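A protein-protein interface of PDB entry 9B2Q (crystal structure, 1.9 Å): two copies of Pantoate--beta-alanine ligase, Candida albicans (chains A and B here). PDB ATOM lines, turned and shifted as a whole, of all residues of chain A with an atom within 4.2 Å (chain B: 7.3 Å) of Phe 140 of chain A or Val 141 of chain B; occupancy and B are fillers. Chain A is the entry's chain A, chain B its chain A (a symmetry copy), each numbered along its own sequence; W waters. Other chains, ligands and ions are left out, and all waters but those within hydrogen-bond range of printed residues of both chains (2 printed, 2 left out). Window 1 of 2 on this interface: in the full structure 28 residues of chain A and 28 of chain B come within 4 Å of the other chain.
The backbone carbonyl oxygen of Gly 138 of chain A lies within hydrogen-bond range of the backbone NH of His 144 of chain B. The backbone NH (N) of Ala 139 of chain A sits at hydrogen-bond distance from the side-chain carboxylate (OD2) of Asp 197 of chain B (3.0 Å). The backbone NH (N) of Phe 140 of chain A sits at hydrogen-bond distance from the backbone carbonyl oxygen (O) of Thr 142 of chain B, 3.0 Å away. NH2 of Arg 160 of chain A lies within hydrogen-bond range of NE2 of His 144 of chain B, at 3.3 Å. O of Gly 138 of chain A sits close to O of Thr 142 of chain B (3.2 Å).
The side-chain amide oxygen (OE1) of Gln 136 of chain A lies within hydrogen-bond range of the guanidinium group (NH1) of Arg 160 of chain A (2.9 Å). N of Val 141 of chain A is in hydrogen-bond range of OG1 of Thr 164 of chain A (2.9 Å). OG1 of Thr 164 of chain A sits at hydrogen-bond distance from O of Arg 160 of chain A. OG1 of Thr 164 of chain B sits at hydrogen-bond distance from N of Val 141 of chain B, at 2.9 Å. The side-chain hydroxyl of Ser 147 of chain B is in hydrogen-bond range of the backbone carbonyl oxygen of Val 143 of chain B.
Among the printed residues, pairs that only touch across the chains: Arg 137 of chain A with His 144 of chain B (3.7 Å), Gly 138 of chain A with Val 143 of chain B (3.6 Å), Gly 138 of chain A with Asp 197 of chain B (3.0 Å), Ala 139 of chain A with Thr 142 of chain B (3.3 Å), Ala 139 of chain A with Leu 198 of chain B (3.9 Å), Phe 140 of chain A with Phe 140 of chain B (3.9 Å), Phe 140 of chain A with Val 141 of chain B (3.4 Å), Phe 140 of chain A with His 144 of chain B (3.7 Å) and Val 141 of chain A with Phe 140 of chain B (3.4 Å).
Of chain B, only Phe 140 (3.9 Å), Val 141 (3.4 Å), Thr 142 (3.0 Å) and His 144 (3.7 Å) come within 4 Å of Phe 140 of chain A. Val 141 of chain B touches just one residue of chain A: Phe 140. Printed residues of chain A within 4 Å of Val 143 of chain B: Gly 138. Of the printed residues of chain A, Asp 197 of chain B touches Gly 138 and Ala 139. Of the printed residues of chain B, Val 141 of chain A touches Phe 140. Of the printed residues of chain A, Phe 140 of chain B touches Phe 140 (3.9 Å) and Val 141 (3.4 Å). Phe 159 of chain B touches none of the printed residues of chain A. The nearest residue of chain B that does not touch Phe 140 of chain A is Val 143 of chain B (5.0 Å). The nearest residue of chain A that does not touch Val 141 of chain B is Val 141 of chain A (4.1 Å). The nearest printed residue of chain B that does not touch Arg 137 of chain A is Asp 197 of chain B (4.9 Å).
Of the 20 printed residues of chain B, 7 touch a printed residue of chain A. Hydrophobic or aromatic side chains of chain B that line the printed part of chain A: Val 141, His 144 and Leu 198. Of the 10 printed residues of chain A, 6 touch a printed residue of chain B. Hydrophobic or aromatic side chains of chain A within 4 Å of the printed part of chain B: Ala 139, Phe 140 and Val 141. Among the printed residues, no Asp or Glu carboxylate lies within 4 Å of a Lys or Arg side-chain nitrogen of the other chain.
Phe 140 of chain A touches its own counterpart, Phe 140 of chain B. Phe 140 of chain A touches Val 141 of chain B, and with the chains exchanged Val 141 of chain A touches Phe 140 of chain B.
Water W2 lies within hydrogen-bond range of O of His 144 of chain B and NH2 of Arg 137 of chain A. Water W1 lies within hydrogen-bond range of a ring nitrogen (NE2) of His 144 of chain B and the guanidinium group of Arg 160 of chain A.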
ATOM      1  N   SER A  78     -19.808   2.117 -18.487  1.00  0.00           N
ATOM      2  CA  SER A  78     -20.427   1.261 -19.506  1.00  0.00           C
ATOM      3  C   SER A  78     -21.629   0.472 -18.991  1.00  0.00           C
ATOM      4  O   SER A  78     -22.333  -0.148 -19.795  1.00  0.00           O
ATOM      5  CB  SER A  78     -19.396   0.303 -20.103  1.00  0.00           C
ATOM      6  OG  SER A  78     -19.002  -0.682 -19.172  1.00  0.00           O
ATOM      7  N   ILE A 129     -14.761   5.661 -24.087  1.00  0.00           N
ATOM      8  CA  ILE A 129     -16.027   5.049 -23.699  1.00  0.00           C
ATOM      9  C   ILE A 129     -17.152   6.033 -23.989  1.00  0.00           C
ATOM     10  O   ILE A 129     -17.000   7.248 -23.823  1.00  0.00           O
ATOM     11  CB  ILE A 129     -16.017   4.604 -22.215  1.00  0.00           C
ATOM     12  CG1 ILE A 129     -17.307   3.852 -21.842  1.00  0.00           C
ATOM     13  CG2 ILE A 129     -15.777   5.797 -21.286  1.00  0.00           C
ATOM     14  CD1 ILE A 129     -17.571   2.581 -22.684  1.00  0.00           C
ATOM     15  N   GLN A 136     -19.453   2.890 -29.432  1.00  0.00           N
ATOM     16  CA  GLN A 136     -18.454   2.273 -28.575  1.00  0.00           C
ATOM     17  C   GLN A 136     -17.359   1.638 -29.419  1.00  0.00           C
ATOM     18  O   GLN A 136     -17.576   1.221 -30.561  1.00  0.00           O
ATOM     19  CB  GLN A 136     -19.098   1.246 -27.642  1.00  0.00           C
ATOM     20  CG  GLN A 136     -19.798   1.934 -26.442  1.00  0.00           C
ATOM     21  CD  GLN A 136     -20.545   0.974 -25.533  1.00  0.00           C
ATOM     22  OE1 GLN A 136     -20.721  -0.200 -25.857  1.00  0.00           O
ATOM     23  NE2 GLN A 136     -21.009   1.480 -24.389  1.00  0.00           N
ATOM     24  N   ARG A 137     -16.166   1.588 -28.840  1.00  0.00           N
ATOM     25  CA  ARG A 137     -14.992   1.078 -29.522  1.00  0.00           C
ATOM     26  C   ARG A 137     -14.163   0.319 -28.500  1.00  0.00           C
ATOM     27  O   ARG A 137     -14.074   0.727 -27.333  1.00  0.00           O
ATOM     28  CB  ARG A 137     -14.179   2.216 -30.153  1.00  0.00           C
ATOM     29  CG  ARG A 137     -12.847   1.768 -30.690  1.00  0.00           C
ATOM     30  CD  ARG A 137     -12.013   2.904 -31.233  1.00  0.00           C
ATOM     31  NE  ARG A 137     -10.712   2.383 -31.631  1.00  0.00           N
ATOM     32  CZ  ARG A 137     -10.471   1.782 -32.788  1.00  0.00           C
ATOM     33  NH1 ARG A 137     -11.402   1.693 -33.729  1.00  0.00           N
ATOM     34  NH2 ARG A 137      -9.272   1.255 -33.005  1.00  0.00           N
ATOM     35  N   GLY A 138     -13.599  -0.801 -28.928  1.00  0.00           N
ATOM     36  CA  GLY A 138     -12.666  -1.568 -28.119  1.00  0.00           C
ATOM     37  C   GLY A 138     -13.265  -2.878 -27.636  1.00  0.00           C
ATOM     38  O   GLY A 138     -14.356  -3.287 -28.040  1.00  0.00           O
ATOM     39  N   ALA A 139     -12.536  -3.533 -26.725  1.00  0.00           N
ATOM     40  CA  ALA A 139     -12.943  -4.849 -26.242  1.00  0.00           C
ATOM     41  C   ALA A 139     -14.060  -4.737 -25.214  1.00  0.00           C
ATOM     42  O   ALA A 139     -13.919  -4.042 -24.193  1.00  0.00           O
ATOM     43  CB  ALA A 139     -11.753  -5.613 -25.628  1.00  0.00           C
ATOM     44  N   PHE A 140     -15.148  -5.475 -25.456  1.00  0.00           N
ATOM     45  CA  PHE A 140     -16.246  -5.611 -24.507  1.00  0.00           C
ATOM     46  C   PHE A 140     -16.584  -7.087 -24.341  1.00  0.00           C
ATOM     47  O   PHE A 140     -16.422  -7.876 -25.269  1.00  0.00           O
ATOM     48  CB  PHE A 140     -17.512  -4.844 -24.968  1.00  0.00           C
ATOM     49  CG  PHE A 140     -17.393  -3.351 -24.843  1.00  0.00           C
ATOM     50  CD1 PHE A 140     -16.656  -2.628 -25.763  1.00  0.00           C
ATOM     51  CD2 PHE A 140     -18.008  -2.680 -23.790  1.00  0.00           C
ATOM     52  CE1 PHE A 140     -16.527  -1.242 -25.654  1.00  0.00           C
ATOM     53  CE2 PHE A 140     -17.893  -1.291 -23.658  1.00  0.00           C
ATOM     54  CZ  PHE A 140     -17.157  -0.570 -24.595  1.00  0.00           C
ATOM     55  N   VAL A 141     -17.056  -7.451 -23.150  1.00  0.00           N
ATOM     56  CA  VAL A 141     -17.381  -8.831 -22.812  1.00  0.00           C
ATOM     57  C   VAL A 141     -18.874  -8.927 -22.549  1.00  0.00           C
ATOM     58  O   VAL A 141     -19.418  -8.127 -21.780  1.00  0.00           O
ATOM     59  CB  VAL A 141     -16.597  -9.307 -21.569  1.00  0.00           C
ATOM     60  CG1 VAL A 141     -16.913 -10.765 -21.281  1.00  0.00           C
ATOM     61  CG2 VAL A 141     -15.119  -9.089 -21.758  1.00  0.00           C
ATOM     62  N   ARG A 160     -23.493  -6.485 -19.648  1.00  0.00           N
ATOM     63  CA  ARG A 160     -22.320  -6.342 -20.511  1.00  0.00           C
ATOM     64  C   ARG A 160     -21.349  -5.318 -19.931  1.00  0.00           C
ATOM     65  O   ARG A 160     -20.132  -5.536 -19.924  1.00  0.00           O
ATOM     66  CB  ARG A 160     -22.751  -5.939 -21.926  1.00  0.00           C
ATOM     67  CG  ARG A 160     -21.593  -5.591 -22.905  1.00  0.00           C
ATOM     68  CD  ARG A 160     -22.215  -5.409 -24.334  1.00  0.00           C
ATOM     69  NE  ARG A 160     -21.303  -4.846 -25.328  1.00  0.00           N
ATOM     70  CZ  ARG A 160     -21.114  -3.543 -25.505  1.00  0.00           C
ATOM     71  NH1 ARG A 160     -21.675  -2.649 -24.702  1.00  0.00           N
ATOM     72  NH2 ARG A 160     -20.364  -3.124 -26.524  1.00  0.00           N
ATOM     73  N   THR A 164     -17.660  -6.489 -18.603  1.00  0.00           N
ATOM     74  CA  THR A 164     -16.517  -5.813 -19.206  1.00  0.00           C
ATOM     75  C   THR A 164     -15.620  -5.196 -18.133  1.00  0.00           C
ATOM     76  O   THR A 164     -14.398  -5.384 -18.144  1.00  0.00           O
ATOM     77  CB  THR A 164     -17.004  -4.736 -20.185  1.00  0.00           C
ATOM     78  OG1 THR A 164     -17.690  -5.355 -21.278  1.00  0.00           O
ATOM     79  CG2 THR A 164     -15.830  -3.930 -20.721  1.00  0.00           C
ATOM     80  N   GLY B 138     -22.778 -17.959 -23.023  1.00  0.00           N
ATOM     81  CA  GLY B 138     -21.578 -17.778 -22.222  1.00  0.00           C
ATOM     82  C   GLY B 138     -20.826 -16.510 -22.589  1.00  0.00           C
ATOM     83  O   GLY B 138     -21.295 -15.673 -23.363  1.00  0.00           O
ATOM     84  N   ALA B 139     -19.614 -16.390 -22.035  1.00  0.00           N
ATOM     85  CA  ALA B 139     -18.819 -15.181 -22.225  1.00  0.00           C
ATOM     86  C   ALA B 139     -18.153 -15.169 -23.595  1.00  0.00           C
ATOM     87  O   ALA B 139     -17.418 -16.104 -23.954  1.00  0.00           O
ATOM     88  CB  ALA B 139     -17.743 -15.040 -21.129  1.00  0.00           C
ATOM     89  N   PHE B 140     -18.363 -14.073 -24.331  1.00  0.00           N
ATOM     90  CA  PHE B 140     -17.683 -13.823 -25.596  1.00  0.00           C
ATOM     91  C   PHE B 140     -17.110 -12.412 -25.585  1.00  0.00           C
ATOM     92  O   PHE B 140     -17.663 -11.515 -24.952  1.00  0.00           O
ATOM     93  CB  PHE B 140     -18.636 -13.979 -26.810  1.00  0.00           C
ATOM     94  CG  PHE B 140     -18.995 -15.406 -27.116  1.00  0.00           C
ATOM     95  CD1 PHE B 140     -19.922 -16.077 -26.339  1.00  0.00           C
ATOM     96  CD2 PHE B 140     -18.386 -16.075 -28.174  1.00  0.00           C
ATOM     97  CE1 PHE B 140     -20.258 -17.405 -26.604  1.00  0.00           C
ATOM     98  CE2 PHE B 140     -18.705 -17.408 -28.459  1.00  0.00           C
ATOM     99  CZ  PHE B 140     -19.647 -18.072 -27.678  1.00  0.00           C
ATOM    100  N   VAL B 141     -15.998 -12.223 -26.292  1.00  0.00           N
ATOM    101  CA  VAL B 141     -15.296 -10.947 -26.346  1.00  0.00           C
ATOM    102  C   VAL B 141     -15.344 -10.426 -27.773  1.00  0.00           C
ATOM    103  O   VAL B 141     -15.024 -11.166 -28.710  1.00  0.00           O
ATOM    104  CB  VAL B 141     -13.827 -11.091 -25.889  1.00  0.00           C
ATOM    105  CG1 VAL B 141     -13.143  -9.734 -25.899  1.00  0.00           C
ATOM    106  CG2 VAL B 141     -13.755 -11.736 -24.530  1.00  0.00           C
ATOM    107  N   THR B 142     -15.740  -9.157 -27.941  1.00  0.00           N
ATOM    108  CA  THR B 142     -15.675  -8.488 -29.235  1.00  0.00           C
ATOM    109  C   THR B 142     -14.805  -7.251 -29.127  1.00  0.00           C
ATOM    110  O   THR B 142     -15.051  -6.399 -28.266  1.00  0.00           O
ATOM    111  CB  THR B 142     -17.066  -8.056 -29.736  1.00  0.00           C
ATOM    112  OG1 THR B 142     -17.967  -9.160 -29.653  1.00  0.00           O
ATOM    113  CG2 THR B 142     -16.970  -7.574 -31.176  1.00  0.00           C
ATOM    114  N   VAL B 143     -13.849  -7.107 -30.037  1.00  0.00           N
ATOM    115  CA  VAL B 143     -13.025  -5.899 -30.108  1.00  0.00           C
ATOM    116  C   VAL B 143     -13.697  -5.024 -31.161  1.00  0.00           C
ATOM    117  O   VAL B 143     -13.423  -5.124 -32.364  1.00  0.00           O
ATOM    118  CB  VAL B 143     -11.557  -6.203 -30.434  1.00  0.00           C
ATOM    119  CG1 VAL B 143     -10.728  -4.904 -30.451  1.00  0.00           C
ATOM    120  CG2 VAL B 143     -10.948  -7.166 -29.392  1.00  0.00           C
ATOM    121  N   HIS B 144     -14.642  -4.204 -30.709  1.00  0.00           N
ATOM    122  CA  HIS B 144     -15.399  -3.351 -31.618  1.00  0.00           C
ATOM    123  C   HIS B 144     -14.480  -2.323 -32.272  1.00  0.00           C
ATOM    124  O   HIS B 144     -13.625  -1.732 -31.612  1.00  0.00           O
ATOM    125  CB  HIS B 144     -16.525  -2.631 -30.842  1.00  0.00           C
ATOM    126  CG  HIS B 144     -17.562  -3.551 -30.265  1.00  0.00           C
ATOM    127  ND1 HIS B 144     -18.531  -4.163 -31.035  1.00  0.00           N
ATOM    128  CD2 HIS B 144     -17.790  -3.951 -28.990  1.00  0.00           C
ATOM    129  CE1 HIS B 144     -19.303  -4.907 -30.263  1.00  0.00           C
ATOM    130  NE2 HIS B 144     -18.877  -4.793 -29.016  1.00  0.00           N
ATOM    131  N   SER B 147     -12.832  -5.201 -35.973  1.00  0.00           N
ATOM    132  CA  SER B 147     -13.314  -6.533 -36.329  1.00  0.00           C
ATOM    133  C   SER B 147     -14.189  -6.557 -37.573  1.00  0.00           C
ATOM    134  O   SER B 147     -14.448  -7.645 -38.109  1.00  0.00           O
ATOM    135  CB  SER B 147     -14.104  -7.136 -35.154  1.00  0.00           C
ATOM    136  OG  SER B 147     -13.247  -7.274 -34.001  1.00  0.00           O
ATOM    137  N   PHE B 159     -13.470 -12.308 -36.058  1.00  0.00           N
ATOM    138  CA  PHE B 159     -12.566 -11.765 -35.045  1.00  0.00           C
ATOM    139  C   PHE B 159     -13.166 -11.770 -33.644  1.00  0.00           C
ATOM    140  O   PHE B 159     -12.410 -11.713 -32.666  1.00  0.00           O
ATOM    141  CB  PHE B 159     -12.107 -10.360 -35.444  1.00  0.00           C
ATOM    142  CG  PHE B 159     -11.150 -10.375 -36.600  1.00  0.00           C
ATOM    143  CD1 PHE B 159      -9.886 -10.943 -36.451  1.00  0.00           C
ATOM    144  CD2 PHE B 159     -11.521  -9.881 -37.843  1.00  0.00           C
ATOM    145  CE1 PHE B 159      -8.992 -10.992 -37.528  1.00  0.00           C
ATOM    146  CE2 PHE B 159     -10.627  -9.927 -38.923  1.00  0.00           C
ATOM    147  CZ  PHE B 159      -9.373 -10.488 -38.763  1.00  0.00           C
ATOM    148  N   ARG B 160     -14.495 -11.832 -33.519  1.00  0.00           N
ATOM    149  CA  ARG B 160     -15.082 -12.136 -32.213  1.00  0.00           C
ATOM    150  C   ARG B 160     -14.683 -13.537 -31.759  1.00  0.00           C
ATOM    151  O   ARG B 160     -14.341 -13.748 -30.590  1.00  0.00           O
ATOM    152  CB  ARG B 160     -16.607 -12.001 -32.275  1.00  0.00           C
ATOM    153  CG  ARG B 160     -17.372 -12.457 -31.000  1.00  0.00           C
ATOM    154  CD  ARG B 160     -18.879 -12.053 -31.176  1.00  0.00           C
ATOM    155  NE  ARG B 160     -19.783 -12.618 -30.176  1.00  0.00           N
ATOM    156  CZ  ARG B 160     -20.340 -13.820 -30.277  1.00  0.00           C
ATOM    157  NH1 ARG B 160     -20.023 -14.647 -31.265  1.00  0.00           N
ATOM    158  NH2 ARG B 160     -21.253 -14.194 -29.382  1.00  0.00           N
ATOM    159  N   GLY B 161     -14.717 -14.509 -32.677  1.00  0.00           N
ATOM    160  CA  GLY B 161     -14.233 -15.843 -32.336  1.00  0.00           C
ATOM    161  C   GLY B 161     -12.778 -15.835 -31.905  1.00  0.00           C
ATOM    162  O   GLY B 161     -12.408 -16.463 -30.904  1.00  0.00           O
ATOM    163  N   VAL B 162     -11.930 -15.135 -32.664  1.00  0.00           N
ATOM    164  CA  VAL B 162     -10.506 -15.058 -32.344  1.00  0.00           C
ATOM    165  C   VAL B 162     -10.289 -14.395 -30.983  1.00  0.00           C
ATOM    166  O   VAL B 162      -9.545 -14.907 -30.130  1.00  0.00           O
ATOM    167  CB  VAL B 162      -9.748 -14.303 -33.446  1.00  0.00           C
ATOM    168  CG1 VAL B 162      -8.309 -14.016 -32.967  1.00  0.00           C
ATOM    169  CG2 VAL B 162      -9.768 -15.092 -34.778  1.00  0.00           C
ATOM    170  N   ALA B 163     -10.903 -13.231 -30.767  1.00  0.00           N
ATOM    171  CA  ALA B 163     -10.680 -12.518 -29.504  1.00  0.00           C
ATOM    172  C   ALA B 163     -11.165 -13.335 -28.315  1.00  0.00           C
ATOM    173  O   ALA B 163     -10.543 -13.324 -27.237  1.00  0.00           O
ATOM    174  CB  ALA B 163     -11.376 -11.159 -29.524  1.00  0.00           C
ATOM    175  N   THR B 164     -12.278 -14.043 -28.488  1.00  0.00           N
ATOM    176  CA  THR B 164     -12.811 -14.887 -27.425  1.00  0.00           C
ATOM    177  C   THR B 164     -11.840 -16.018 -27.088  1.00  0.00           C
ATOM    178  O   THR B 164     -11.523 -16.253 -25.915  1.00  0.00           O
ATOM    179  CB  THR B 164     -14.174 -15.454 -27.842  1.00  0.00           C
ATOM    180  OG1 THR B 164     -15.118 -14.387 -27.978  1.00  0.00           O
ATOM    181  CG2 THR B 164     -14.683 -16.443 -26.803  1.00  0.00           C
ATOM    182  N   VAL B 165     -11.340 -16.728 -28.100  1.00  0.00           N
ATOM    183  CA  VAL B 165     -10.476 -17.867 -27.754  1.00  0.00           C
ATOM    184  C   VAL B 165      -9.101 -17.402 -27.268  1.00  0.00           C
ATOM    185  O   VAL B 165      -8.506 -18.038 -26.378  1.00  0.00           O
ATOM    186  CB  VAL B 165     -10.381 -18.871 -28.926  1.00  0.00           C
ATOM    187  CG1 VAL B 165      -9.441 -18.381 -30.042  1.00  0.00           C
ATOM    188  CG2 VAL B 165      -9.951 -20.269 -28.395  1.00  0.00           C
ATOM    189  N   THR B 167      -8.530 -14.741 -25.506  1.00  0.00           N
ATOM    190  CA  THR B 167      -8.750 -14.367 -24.109  1.00  0.00           C
ATOM    191  C   THR B 167      -8.710 -15.601 -23.210  1.00  0.00           C
ATOM    192  O   THR B 167      -8.040 -15.606 -22.170  1.00  0.00           O
ATOM    193  CB  THR B 167     -10.085 -13.621 -23.948  1.00  0.00           C
ATOM    194  OG1 THR B 167     -10.032 -12.398 -24.684  1.00  0.00           O
ATOM    195  CG2 THR B 167     -10.321 -13.253 -22.465  1.00  0.00           C
ATOM    196  N   LYS B 168      -9.424 -16.666 -23.600  1.00  0.00           N
ATOM    197  CA  LYS B 168      -9.402 -17.901 -22.812  1.00  0.00           C
ATOM    198  C   LYS B 168      -7.986 -18.466 -22.693  1.00  0.00           C
ATOM    199  O   LYS B 168      -7.552 -18.861 -21.604  1.00  0.00           O
ATOM    200  CB  LYS B 168     -10.338 -18.942 -23.446  1.00  0.00           C
ATOM    201  CG  LYS B 168     -11.865 -18.584 -23.372  1.00  0.00           C
ATOM    202  CD  LYS B 168     -12.623 -19.423 -24.437  1.00  0.00           C
ATOM    203  CE  LYS B 168     -14.138 -19.154 -24.457  1.00  0.00           C
ATOM    204  NZ  LYS B 168     -14.924 -20.034 -23.509  1.00  0.00           N
ATOM    205  N   LEU B 194      -7.149  -5.995 -27.911  1.00  0.00           N
ATOM    206  CA  LEU B 194      -7.657  -6.874 -26.856  1.00  0.00           C
ATOM    207  C   LEU B 194      -6.830  -6.735 -25.578  1.00  0.00           C
ATOM    208  O   LEU B 194      -7.366  -6.549 -24.481  1.00  0.00           O
ATOM    209  CB  LEU B 194      -7.618  -8.333 -27.332  1.00  0.00           C
ATOM    210  CG  LEU B 194      -8.031  -9.416 -26.333  1.00  0.00           C
ATOM    211  CD1 LEU B 194      -9.545  -9.321 -26.053  1.00  0.00           C
ATOM    212  CD2 LEU B 194      -7.678 -10.807 -26.855  1.00  0.00           C
ATOM    213  N   ASP B 197      -7.149  -3.161 -24.130  1.00  0.00           N
ATOM    214  CA  ASP B 197      -8.456  -2.768 -23.605  1.00  0.00           C
ATOM    215  C   ASP B 197      -8.884  -3.608 -22.412  1.00  0.00           C
ATOM    216  O   ASP B 197      -9.559  -3.099 -21.507  1.00  0.00           O
ATOM    217  CB  ASP B 197      -9.528  -2.863 -24.701  1.00  0.00           C
ATOM    218  CG  ASP B 197      -9.439  -1.744 -25.706  1.00  0.00           C
ATOM    219  OD1 ASP B 197      -8.836  -0.693 -25.410  1.00  0.00           O
ATOM    220  OD2 ASP B 197      -9.998  -1.909 -26.805  1.00  0.00           O
ATOM    221  N   LEU B 198      -8.564  -4.905 -22.412  1.00  0.00           N
ATOM    222  CA  LEU B 198      -8.834  -5.726 -21.241  1.00  0.00           C
ATOM    223  C   LEU B 198      -7.711  -5.634 -20.215  1.00  0.00           C
ATOM    224  O   LEU B 198      -7.805  -6.254 -19.148  1.00  0.00           O
ATOM    225  CB  LEU B 198      -9.085  -7.190 -21.646  1.00  0.00           C
ATOM    226  CG  LEU B 198     -10.363  -7.415 -22.497  1.00  0.00           C
ATOM    227  CD1 LEU B 198     -10.604  -8.919 -22.694  1.00  0.00           C
ATOM    228  CD2 LEU B 198     -11.604  -6.754 -21.877  1.00  0.00           C
HETATM  229  O   HOH W   1     -20.084  -6.492 -27.311  1.00  0.00           O
HETATM  230  O   HOH W   2     -10.950  -1.486 -31.688  1.00  0.00           O
